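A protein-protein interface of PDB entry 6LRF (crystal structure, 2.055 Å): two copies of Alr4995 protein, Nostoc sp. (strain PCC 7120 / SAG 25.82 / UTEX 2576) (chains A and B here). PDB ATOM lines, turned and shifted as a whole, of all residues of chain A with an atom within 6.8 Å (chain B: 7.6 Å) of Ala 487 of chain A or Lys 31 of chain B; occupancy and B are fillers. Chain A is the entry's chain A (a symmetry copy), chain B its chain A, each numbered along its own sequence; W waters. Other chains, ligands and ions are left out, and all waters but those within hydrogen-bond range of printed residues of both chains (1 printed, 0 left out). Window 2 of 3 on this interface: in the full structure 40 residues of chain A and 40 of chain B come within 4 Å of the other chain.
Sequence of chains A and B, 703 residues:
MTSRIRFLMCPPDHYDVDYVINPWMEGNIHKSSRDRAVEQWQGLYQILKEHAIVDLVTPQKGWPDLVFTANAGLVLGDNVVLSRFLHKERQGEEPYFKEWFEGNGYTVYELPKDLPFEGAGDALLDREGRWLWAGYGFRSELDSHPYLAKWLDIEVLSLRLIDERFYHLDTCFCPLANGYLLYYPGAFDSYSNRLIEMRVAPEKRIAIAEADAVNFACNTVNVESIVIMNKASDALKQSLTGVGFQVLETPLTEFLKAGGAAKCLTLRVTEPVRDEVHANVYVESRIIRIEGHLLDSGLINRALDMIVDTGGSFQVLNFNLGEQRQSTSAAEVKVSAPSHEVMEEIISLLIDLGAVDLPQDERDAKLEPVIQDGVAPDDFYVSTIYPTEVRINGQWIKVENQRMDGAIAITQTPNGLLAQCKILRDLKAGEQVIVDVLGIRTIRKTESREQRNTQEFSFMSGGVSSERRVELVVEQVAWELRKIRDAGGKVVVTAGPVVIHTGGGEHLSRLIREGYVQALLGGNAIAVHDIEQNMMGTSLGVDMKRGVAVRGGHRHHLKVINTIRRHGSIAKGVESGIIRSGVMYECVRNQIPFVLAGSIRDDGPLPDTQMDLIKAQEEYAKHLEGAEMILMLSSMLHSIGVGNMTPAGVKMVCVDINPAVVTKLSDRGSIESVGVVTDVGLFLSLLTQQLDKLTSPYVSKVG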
ATOM      1  N   ARG A 482      22.151  11.125  -8.124  1.00  0.00           N
ATOM      2  CA  ARG A 482      21.148  11.161  -7.056  1.00  0.00           C
ATOM      3  C   ARG A 482      21.461  12.322  -6.140  1.00  0.00           C
ATOM      4  O   ARG A 482      20.568  13.051  -5.710  1.00  0.00           O
ATOM      5  CB  ARG A 482      21.116   9.839  -6.278  1.00  0.00           C
ATOM      6  CG  ARG A 482      20.310   9.859  -4.952  1.00  0.00           C
ATOM      7  CD  ARG A 482      20.161   8.440  -4.380  1.00  0.00           C
ATOM      8  NE  ARG A 482      20.057   8.358  -2.913  1.00  0.00           N
ATOM      9  CZ  ARG A 482      21.100   8.353  -2.076  1.00  0.00           C
ATOM     10  NH1 ARG A 482      22.348   8.453  -2.544  1.00  0.00           N
ATOM     11  NH2 ARG A 482      20.904   8.257  -0.761  1.00  0.00           N
ATOM     12  N   LYS A 483      22.749  12.510  -5.881  1.00  0.00           N
ATOM     13  CA  LYS A 483      23.195  13.609  -5.044  1.00  0.00           C
ATOM     14  C   LYS A 483      22.818  14.962  -5.653  1.00  0.00           C
ATOM     15  O   LYS A 483      22.259  15.824  -4.978  1.00  0.00           O
ATOM     16  CB  LYS A 483      24.700  13.496  -4.839  1.00  0.00           C
ATOM     17  CG  LYS A 483      25.309  14.538  -3.968  1.00  0.00           C
ATOM     18  CD  LYS A 483      26.780  14.186  -3.770  1.00  0.00           C
ATOM     19  CE  LYS A 483      27.382  15.048  -2.718  1.00  0.00           C
ATOM     20  NZ  LYS A 483      27.301  16.444  -3.168  1.00  0.00           N
ATOM     21  N   ILE A 484      23.124  15.158  -6.929  1.00  0.00           N
ATOM     22  CA  ILE A 484      22.796  16.429  -7.575  1.00  0.00           C
ATOM     23  C   ILE A 484      21.280  16.665  -7.639  1.00  0.00           C
ATOM     24  O   ILE A 484      20.819  17.757  -7.341  1.00  0.00           O
ATOM     25  CB  ILE A 484      23.371  16.504  -9.000  1.00  0.00           C
ATOM     26  CG1 ILE A 484      24.897  16.545  -8.951  1.00  0.00           C
ATOM     27  CG2 ILE A 484      22.834  17.730  -9.735  1.00  0.00           C
ATOM     28  CD1 ILE A 484      25.527  16.292 -10.304  1.00  0.00           C
ATOM     29  N   ARG A 485      20.513  15.647  -8.039  1.00  0.00           N
ATOM     30  CA  ARG A 485      19.054  15.792  -8.103  1.00  0.00           C
ATOM     31  C   ARG A 485      18.502  16.236  -6.748  1.00  0.00           C
ATOM     32  O   ARG A 485      17.727  17.191  -6.669  1.00  0.00           O
ATOM     33  CB  ARG A 485      18.358  14.486  -8.537  1.00  0.00           C
ATOM     34  CG  ARG A 485      16.800  14.618  -8.581  1.00  0.00           C
ATOM     35  CD  ARG A 485      16.065  13.283  -8.764  1.00  0.00           C
ATOM     36  NE  ARG A 485      16.126  12.432  -7.576  1.00  0.00           N
ATOM     37  CZ  ARG A 485      15.441  11.296  -7.419  1.00  0.00           C
ATOM     38  NH1 ARG A 485      14.621  10.854  -8.369  1.00  0.00           N
ATOM     39  NH2 ARG A 485      15.565  10.600  -6.302  1.00  0.00           N
ATOM     40  N   ASP A 486      18.929  15.555  -5.686  1.00  0.00           N
ATOM     41  CA  ASP A 486      18.447  15.838  -4.336  1.00  0.00           C
ATOM     42  C   ASP A 486      18.800  17.245  -3.846  1.00  0.00           C
ATOM     43  O   ASP A 486      18.074  17.823  -3.038  1.00  0.00           O
ATOM     44  CB  ASP A 486      18.994  14.799  -3.348  1.00  0.00           C
ATOM     45  CG  ASP A 486      18.367  13.402  -3.533  1.00  0.00           C
ATOM     46  OD1 ASP A 486      17.609  13.159  -4.519  1.00  0.00           O
ATOM     47  OD2 ASP A 486      18.660  12.526  -2.682  1.00  0.00           O
ATOM     48  N   ALA A 487      19.899  17.815  -4.335  1.00  0.00           N
ATOM     49  CA  ALA A 487      20.292  19.152  -3.886  1.00  0.00           C
ATOM     50  C   ALA A 487      19.708  20.237  -4.794  1.00  0.00           C
ATOM     51  O   ALA A 487      19.959  21.419  -4.595  1.00  0.00           O
ATOM     52  CB  ALA A 487      21.814  19.269  -3.827  1.00  0.00           C
ATOM     53  N   GLY A 488      18.946  19.827  -5.803  1.00  0.00           N
ATOM     54  CA  GLY A 488      18.358  20.765  -6.750  1.00  0.00           C
ATOM     55  C   GLY A 488      19.354  21.379  -7.719  1.00  0.00           C
ATOM     56  O   GLY A 488      19.151  22.495  -8.195  1.00  0.00           O
ATOM     57  N   GLY A 489      20.432  20.654  -8.012  1.00  0.00           N
ATOM     58  CA  GLY A 489      21.425  21.122  -8.964  1.00  0.00           C
ATOM     59  C   GLY A 489      21.033  20.869 -10.413  1.00  0.00           C
ATOM     60  O   GLY A 489      19.890  20.529 -10.701  1.00  0.00           O
ATOM     61  N   LYS A 490      21.974  21.022 -11.334  1.00  0.00           N
ATOM     62  CA  LYS A 490      21.638  20.954 -12.753  1.00  0.00           C
ATOM     63  C   LYS A 490      22.489  19.938 -13.510  1.00  0.00           C
ATOM     64  O   LYS A 490      23.718  20.019 -13.505  1.00  0.00           O
ATOM     65  CB  LYS A 490      21.772  22.344 -13.379  1.00  0.00           C
ATOM     66  CG  LYS A 490      21.486  22.426 -14.874  1.00  0.00           C
ATOM     67  CD  LYS A 490      21.650  23.861 -15.360  1.00  0.00           C
ATOM     68  CE  LYS A 490      21.072  24.051 -16.761  1.00  0.00           C
ATOM     69  NZ  LYS A 490      21.129  25.473 -17.236  1.00  0.00           N
ATOM     70  N   GLU A 628      26.283  21.350 -13.395  1.00  0.00           N
ATOM     71  CA  GLU A 628      27.215  20.762 -12.447  1.00  0.00           C
ATOM     72  C   GLU A 628      27.775  19.487 -13.038  1.00  0.00           C
ATOM     73  O   GLU A 628      28.880  19.054 -12.703  1.00  0.00           O
ATOM     74  CB  GLU A 628      26.532  20.485 -11.106  1.00  0.00           C
ATOM     75  CG  GLU A 628      26.400  21.723 -10.214  1.00  0.00           C
ATOM     76  CD  GLU A 628      25.405  21.518  -9.078  1.00  0.00           C
ATOM     77  OE1 GLU A 628      24.447  20.748  -9.284  1.00  0.00           O
ATOM     78  OE2 GLU A 628      25.570  22.122  -7.990  1.00  0.00           O
ATOM     79  N   ASP B  16      27.583  25.748   8.141  1.00  0.00           N
ATOM     80  CA  ASP B  16      27.091  25.732   6.766  1.00  0.00           C
ATOM     81  C   ASP B  16      28.166  25.033   5.948  1.00  0.00           C
ATOM     82  O   ASP B  16      29.251  24.745   6.456  1.00  0.00           O
ATOM     83  CB  ASP B  16      26.820  27.150   6.226  1.00  0.00           C
ATOM     84  CG  ASP B  16      25.747  27.186   5.100  1.00  0.00           C
ATOM     85  OD1 ASP B  16      25.384  26.131   4.515  1.00  0.00           O
ATOM     86  OD2 ASP B  16      25.266  28.295   4.785  1.00  0.00           O
ATOM     87  N   VAL B  17      27.870  24.768   4.686  1.00  0.00           N
ATOM     88  CA  VAL B  17      28.897  24.345   3.765  1.00  0.00           C
ATOM     89  C   VAL B  17      29.437  25.605   3.081  1.00  0.00           C
ATOM     90  O   VAL B  17      28.750  26.209   2.257  1.00  0.00           O
ATOM     91  CB  VAL B  17      28.354  23.325   2.752  1.00  0.00           C
ATOM     92  CG1 VAL B  17      29.421  22.939   1.752  1.00  0.00           C
ATOM     93  CG2 VAL B  17      27.815  22.100   3.484  1.00  0.00           C
ATOM     94  N   ASP B  18      30.657  25.990   3.449  1.00  0.00           N
ATOM     95  CA  ASP B  18      31.294  27.228   2.982  1.00  0.00           C
ATOM     96  C   ASP B  18      32.331  26.989   1.913  1.00  0.00           C
ATOM     97  O   ASP B  18      32.750  27.918   1.260  1.00  0.00           O
ATOM     98  CB  ASP B  18      31.986  27.970   4.130  1.00  0.00           C
ATOM     99  CG  ASP B  18      31.000  28.541   5.144  1.00  0.00           C
ATOM    100  OD1 ASP B  18      29.793  28.591   4.828  1.00  0.00           O
ATOM    101  OD2 ASP B  18      31.437  28.950   6.246  1.00  0.00           O
ATOM    102  N   MET B  25      30.608  17.681  -0.014  1.00  0.00           N
ATOM    103  CA  MET B  25      30.424  19.140  -0.030  1.00  0.00           C
ATOM    104  C   MET B  25      30.232  19.689  -1.447  1.00  0.00           C
ATOM    105  O   MET B  25      29.689  20.784  -1.636  1.00  0.00           O
ATOM    106  CB  MET B  25      31.628  19.841   0.615  1.00  0.00           C
ATOM    107  CG  MET B  25      31.797  19.606   2.114  1.00  0.00           C
ATOM    108  SD  MET B  25      33.198  20.735   2.834  1.00  0.00           S
ATOM    109  CE  MET B  25      33.511  19.801   4.540  1.00  0.00           C
ATOM    110  N   GLU B  26      30.687  18.935  -2.444  1.00  0.00           N
ATOM    111  CA  GLU B  26      30.629  19.400  -3.831  1.00  0.00           C
ATOM    112  C   GLU B  26      29.171  19.607  -4.252  1.00  0.00           C
ATOM    113  O   GLU B  26      28.346  18.704  -4.126  1.00  0.00           O
ATOM    114  CB  GLU B  26      31.345  18.407  -4.751  1.00  0.00           C
ATOM    115  CG  GLU B  26      31.467  18.846  -6.215  1.00  0.00           C
ATOM    116  CD  GLU B  26      32.266  20.136  -6.391  1.00  0.00           C
ATOM    117  OE1 GLU B  26      33.518  20.067  -6.415  1.00  0.00           O
ATOM    118  OE2 GLU B  26      31.639  21.222  -6.499  1.00  0.00           O
ATOM    119  N   GLY B  27      28.848  20.809  -4.717  1.00  0.00           N
ATOM    120  CA  GLY B  27      27.482  21.136  -5.090  1.00  0.00           C
ATOM    121  C   GLY B  27      26.647  21.739  -3.967  1.00  0.00           C
ATOM    122  O   GLY B  27      25.530  22.199  -4.203  1.00  0.00           O
ATOM    123  N   ASN B  28      27.187  21.765  -2.749  1.00  0.00           N
ATOM    124  CA  ASN B  28      26.361  22.064  -1.575  1.00  0.00           C
ATOM    125  C   ASN B  28      26.677  23.369  -0.869  1.00  0.00           C
ATOM    126  O   ASN B  28      26.123  23.637   0.200  1.00  0.00           O
ATOM    127  CB  ASN B  28      26.455  20.924  -0.553  1.00  0.00           C
ATOM    128  CG  ASN B  28      25.543  19.771  -0.892  1.00  0.00           C
ATOM    129  OD1 ASN B  28      24.541  19.952  -1.572  1.00  0.00           O
ATOM    130  ND2 ASN B  28      25.901  18.571  -0.445  1.00  0.00           N
ATOM    131  N   ILE B  29      27.543  24.189  -1.455  1.00  0.00           N
ATOM    132  CA  ILE B  29      27.899  25.453  -0.810  1.00  0.00           C
ATOM    133  C   ILE B  29      26.656  26.298  -0.543  1.00  0.00           C
ATOM    134  O   ILE B  29      25.831  26.506  -1.433  1.00  0.00           O
ATOM    135  CB  ILE B  29      28.929  26.263  -1.641  1.00  0.00           C
ATOM    136  CG1 ILE B  29      30.282  25.528  -1.646  1.00  0.00           C
ATOM    137  CG2 ILE B  29      29.077  27.684  -1.071  1.00  0.00           C
ATOM    138  CD1 ILE B  29      31.388  26.233  -2.406  1.00  0.00           C
ATOM    139  N   HIS B  30      26.533  26.731   0.714  1.00  0.00           N
ATOM    140  CA  HIS B  30      25.402  27.502   1.220  1.00  0.00           C
ATOM    141  C   HIS B  30      24.067  26.864   0.877  1.00  0.00           C
ATOM    142  O   HIS B  30      23.096  27.550   0.583  1.00  0.00           O
ATOM    143  CB  HIS B  30      25.467  28.939   0.696  1.00  0.00           C
ATOM    144  CG  HIS B  30      26.700  29.672   1.124  1.00  0.00           C
ATOM    145  ND1 HIS B  30      27.212  30.746   0.427  1.00  0.00           N
ATOM    146  CD2 HIS B  30      27.543  29.466   2.169  1.00  0.00           C
ATOM    147  CE1 HIS B  30      28.301  31.185   1.034  1.00  0.00           C
ATOM    148  NE2 HIS B  30      28.528  30.424   2.091  1.00  0.00           N
ATOM    149  N   LYS B  31      24.022  25.539   0.910  1.00  0.00           N
ATOM    150  CA  LYS B  31      22.773  24.831   0.672  1.00  0.00           C
ATOM    151  C   LYS B  31      22.280  24.147   1.944  1.00  0.00           C
ATOM    152  O   LYS B  31      21.349  23.348   1.905  1.00  0.00           O
ATOM    153  CB  LYS B  31      22.923  23.808  -0.452  1.00  0.00           C
ATOM    154  CG  LYS B  31      22.861  24.425  -1.856  1.00  0.00           C
ATOM    155  CD  LYS B  31      22.517  23.379  -2.916  1.00  0.00           C
ATOM    156  CE  LYS B  31      22.601  23.961  -4.328  1.00  0.00           C
ATOM    157  NZ  LYS B  31      22.130  22.977  -5.357  1.00  0.00           N
ATOM    158  N   SER B  32      22.892  24.471   3.078  1.00  0.00           N
ATOM    159  CA  SER B  32      22.401  23.933   4.337  1.00  0.00           C
ATOM    160  C   SER B  32      21.265  24.768   4.893  1.00  0.00           C
ATOM    161  O   SER B  32      21.317  25.997   4.859  1.00  0.00           O
ATOM    162  CB  SER B  32      23.500  23.852   5.385  1.00  0.00           C
ATOM    163  OG  SER B  32      22.901  23.554   6.639  1.00  0.00           O
ATOM    164  N   SER B  33      20.245  24.093   5.408  1.00  0.00           N
ATOM    165  CA  SER B  33      19.154  24.777   6.101  1.00  0.00           C
ATOM    166  C   SER B  33      19.479  24.897   7.584  1.00  0.00           C
ATOM    167  O   SER B  33      19.648  23.888   8.281  1.00  0.00           O
ATOM    168  CB  SER B  33      17.830  24.037   5.911  1.00  0.00           C
ATOM    169  OG  SER B  33      16.889  24.483   6.876  1.00  0.00           O
ATOM    170  N   ARG B  34      19.583  26.133   8.058  1.00  0.00           N
ATOM    171  CA  ARG B  34      19.952  26.403   9.440  1.00  0.00           C
ATOM    172  C   ARG B  34      18.956  25.793  10.431  1.00  0.00           C
ATOM    173  O   ARG B  34      19.370  25.195  11.418  1.00  0.00           O
ATOM    174  CB  ARG B  34      20.077  27.915   9.673  1.00  0.00           C
ATOM    175  CG  ARG B  34      20.502  28.301  11.104  1.00  0.00           C
ATOM    176  CD  ARG B  34      21.773  27.564  11.586  1.00  0.00           C
ATOM    177  NE  ARG B  34      22.962  27.872  10.784  1.00  0.00           N
ATOM    178  CZ  ARG B  34      23.784  28.899  11.006  1.00  0.00           C
ATOM    179  NH1 ARG B  34      23.552  29.729  12.012  1.00  0.00           N
ATOM    180  NH2 ARG B  34      24.840  29.100  10.219  1.00  0.00           N
ATOM    181  N   ARG B  36      16.782  23.235   9.975  1.00  0.00           N
ATOM    182  CA  ARG B  36      16.774  21.783   9.951  1.00  0.00           C
ATOM    183  C   ARG B  36      18.072  21.262  10.581  1.00  0.00           C
ATOM    184  O   ARG B  36      18.058  20.254  11.293  1.00  0.00           O
ATOM    185  CB  ARG B  36      16.599  21.251   8.529  1.00  0.00           C
ATOM    186  CG  ARG B  36      16.093  19.804   8.465  1.00  0.00           C
ATOM    187  CD  ARG B  36      16.117  19.212   7.045  1.00  0.00           C
ATOM    188  NE  ARG B  36      15.130  19.822   6.148  1.00  0.00           N
ATOM    189  CZ  ARG B  36      15.414  20.687   5.167  1.00  0.00           C
ATOM    190  NH1 ARG B  36      14.429  21.177   4.417  1.00  0.00           N
ATOM    191  NH2 ARG B  36      16.670  21.065   4.921  1.00  0.00           N
ATOM    192  N   GLU B 254      21.300  17.115   6.856  1.00  0.00           N
ATOM    193  CA  GLU B 254      21.956  18.433   6.764  1.00  0.00           C
ATOM    194  C   GLU B 254      23.469  18.347   7.003  1.00  0.00           C
ATOM    195  O   GLU B 254      24.249  19.164   6.480  1.00  0.00           O
ATOM    196  CB  GLU B 254      21.338  19.421   7.760  1.00  0.00           C
ATOM    197  CG  GLU B 254      19.883  19.794   7.431  1.00  0.00           C
ATOM    198  CD  GLU B 254      19.714  20.330   6.007  1.00  0.00           C
ATOM    199  OE1 GLU B 254      20.447  21.268   5.621  1.00  0.00           O
ATOM    200  OE2 GLU B 254      18.848  19.809   5.272  1.00  0.00           O
ATOM    201  N   LYS B 257      25.393  16.639   4.072  1.00  0.00           N
ATOM    202  CA  LYS B 257      25.718  17.595   3.012  1.00  0.00           C
ATOM    203  C   LYS B 257      27.185  18.055   3.105  1.00  0.00           C
ATOM    204  O   LYS B 257      27.763  18.440   2.092  1.00  0.00           O
ATOM    205  CB  LYS B 257      24.785  18.814   3.060  1.00  0.00           C
ATOM    206  CG  LYS B 257      23.329  18.523   2.625  1.00  0.00           C
ATOM    207  CD  LYS B 257      22.486  19.785   2.757  1.00  0.00           C
ATOM    208  CE  LYS B 257      21.001  19.524   2.571  1.00  0.00           C
ATOM    209  NZ  LYS B 257      20.251  20.821   2.710  1.00  0.00           N
HETATM  210  O   HOH W   1      24.936  17.915  -3.735  1.00  0.00           O
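Ala 487 of chain A touches just these residues of chain B: Asn 28 (3.6 Å) and Lys 31 (2.8 Å). Lys 31 of chain B touches three residues of chain A. Of the printed residues of chain B, Lys 483 of chain A touches Glu 26 and Asn 28. Printed residues of chain A within 4 Å of Gly 27 of chain B: Glu 628 (3.6 Å). Ile 29 of chain B touches none of the printed residues of chain A. Asp 16 of chain B touches none of the printed residues of chain A. The nearest printed residue of chain B that does not touch Gly 489 of chain A is Gly 27 of chain B (6.4 Å).
Asn 28 of chain B touches Lys 483 of chain A. OD1 of Asn 28 of chain B touches CB of Ala 487 of chain A, 3.6 Å away. Lys 31 of chain B touches Gly 488 of chain A. Gly 489 of chain A touches Lys 31 of chain B (N to NZ, 3.9 Å). Glu 628 of chain A touches Gly 27 of chain B (OE2 to CA, 3.6 Å).
Of the 16 printed residues of chain B, 4 touch a printed residue of chain A. Among the printed residues, 7 pairs touch across the chains. Among the printed residues, no Asp or Glu carboxylate lies within 4 Å of a Lys or Arg side-chain nitrogen of the other chain.
The side-chain amide nitrogen (ND2) of Asn 28 of chain B is in hydrogen-bond range of the backbone carbonyl oxygen (O) of Lys 257 of chain B (3.1 Å). N of Gly 489 of chain A is in hydrogen-bond range of O of Ile 484 of chain A (3.0 Å). The backbone carbonyl oxygen of Lys 31 of chain B lies within hydrogen-bond range of the side-chain amino group of Lys 257 of chain B, 2.9 Å away. The backbone NH (N) of Glu 628 of chain A lies within hydrogen-bond range of the backbone carbonyl oxygen (O) of Lys 490 of chain A (2.9 Å).
No position is printed for both chains.
Water W1 bridges the side-chain amino group (NZ) of Lys 483 of chain A (2.8 Å) and the side-chain amide oxygen (OD1) of Asn 28 of chain B (3.0 Å).
O of Glu 26 of chain B is in hydrogen-bond range of NZ of Lys 483 of chain A. NZ of Lys 31 of chain B sits at hydrogen-bond distance from O of Ala 487 of chain A (2.8 Å).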
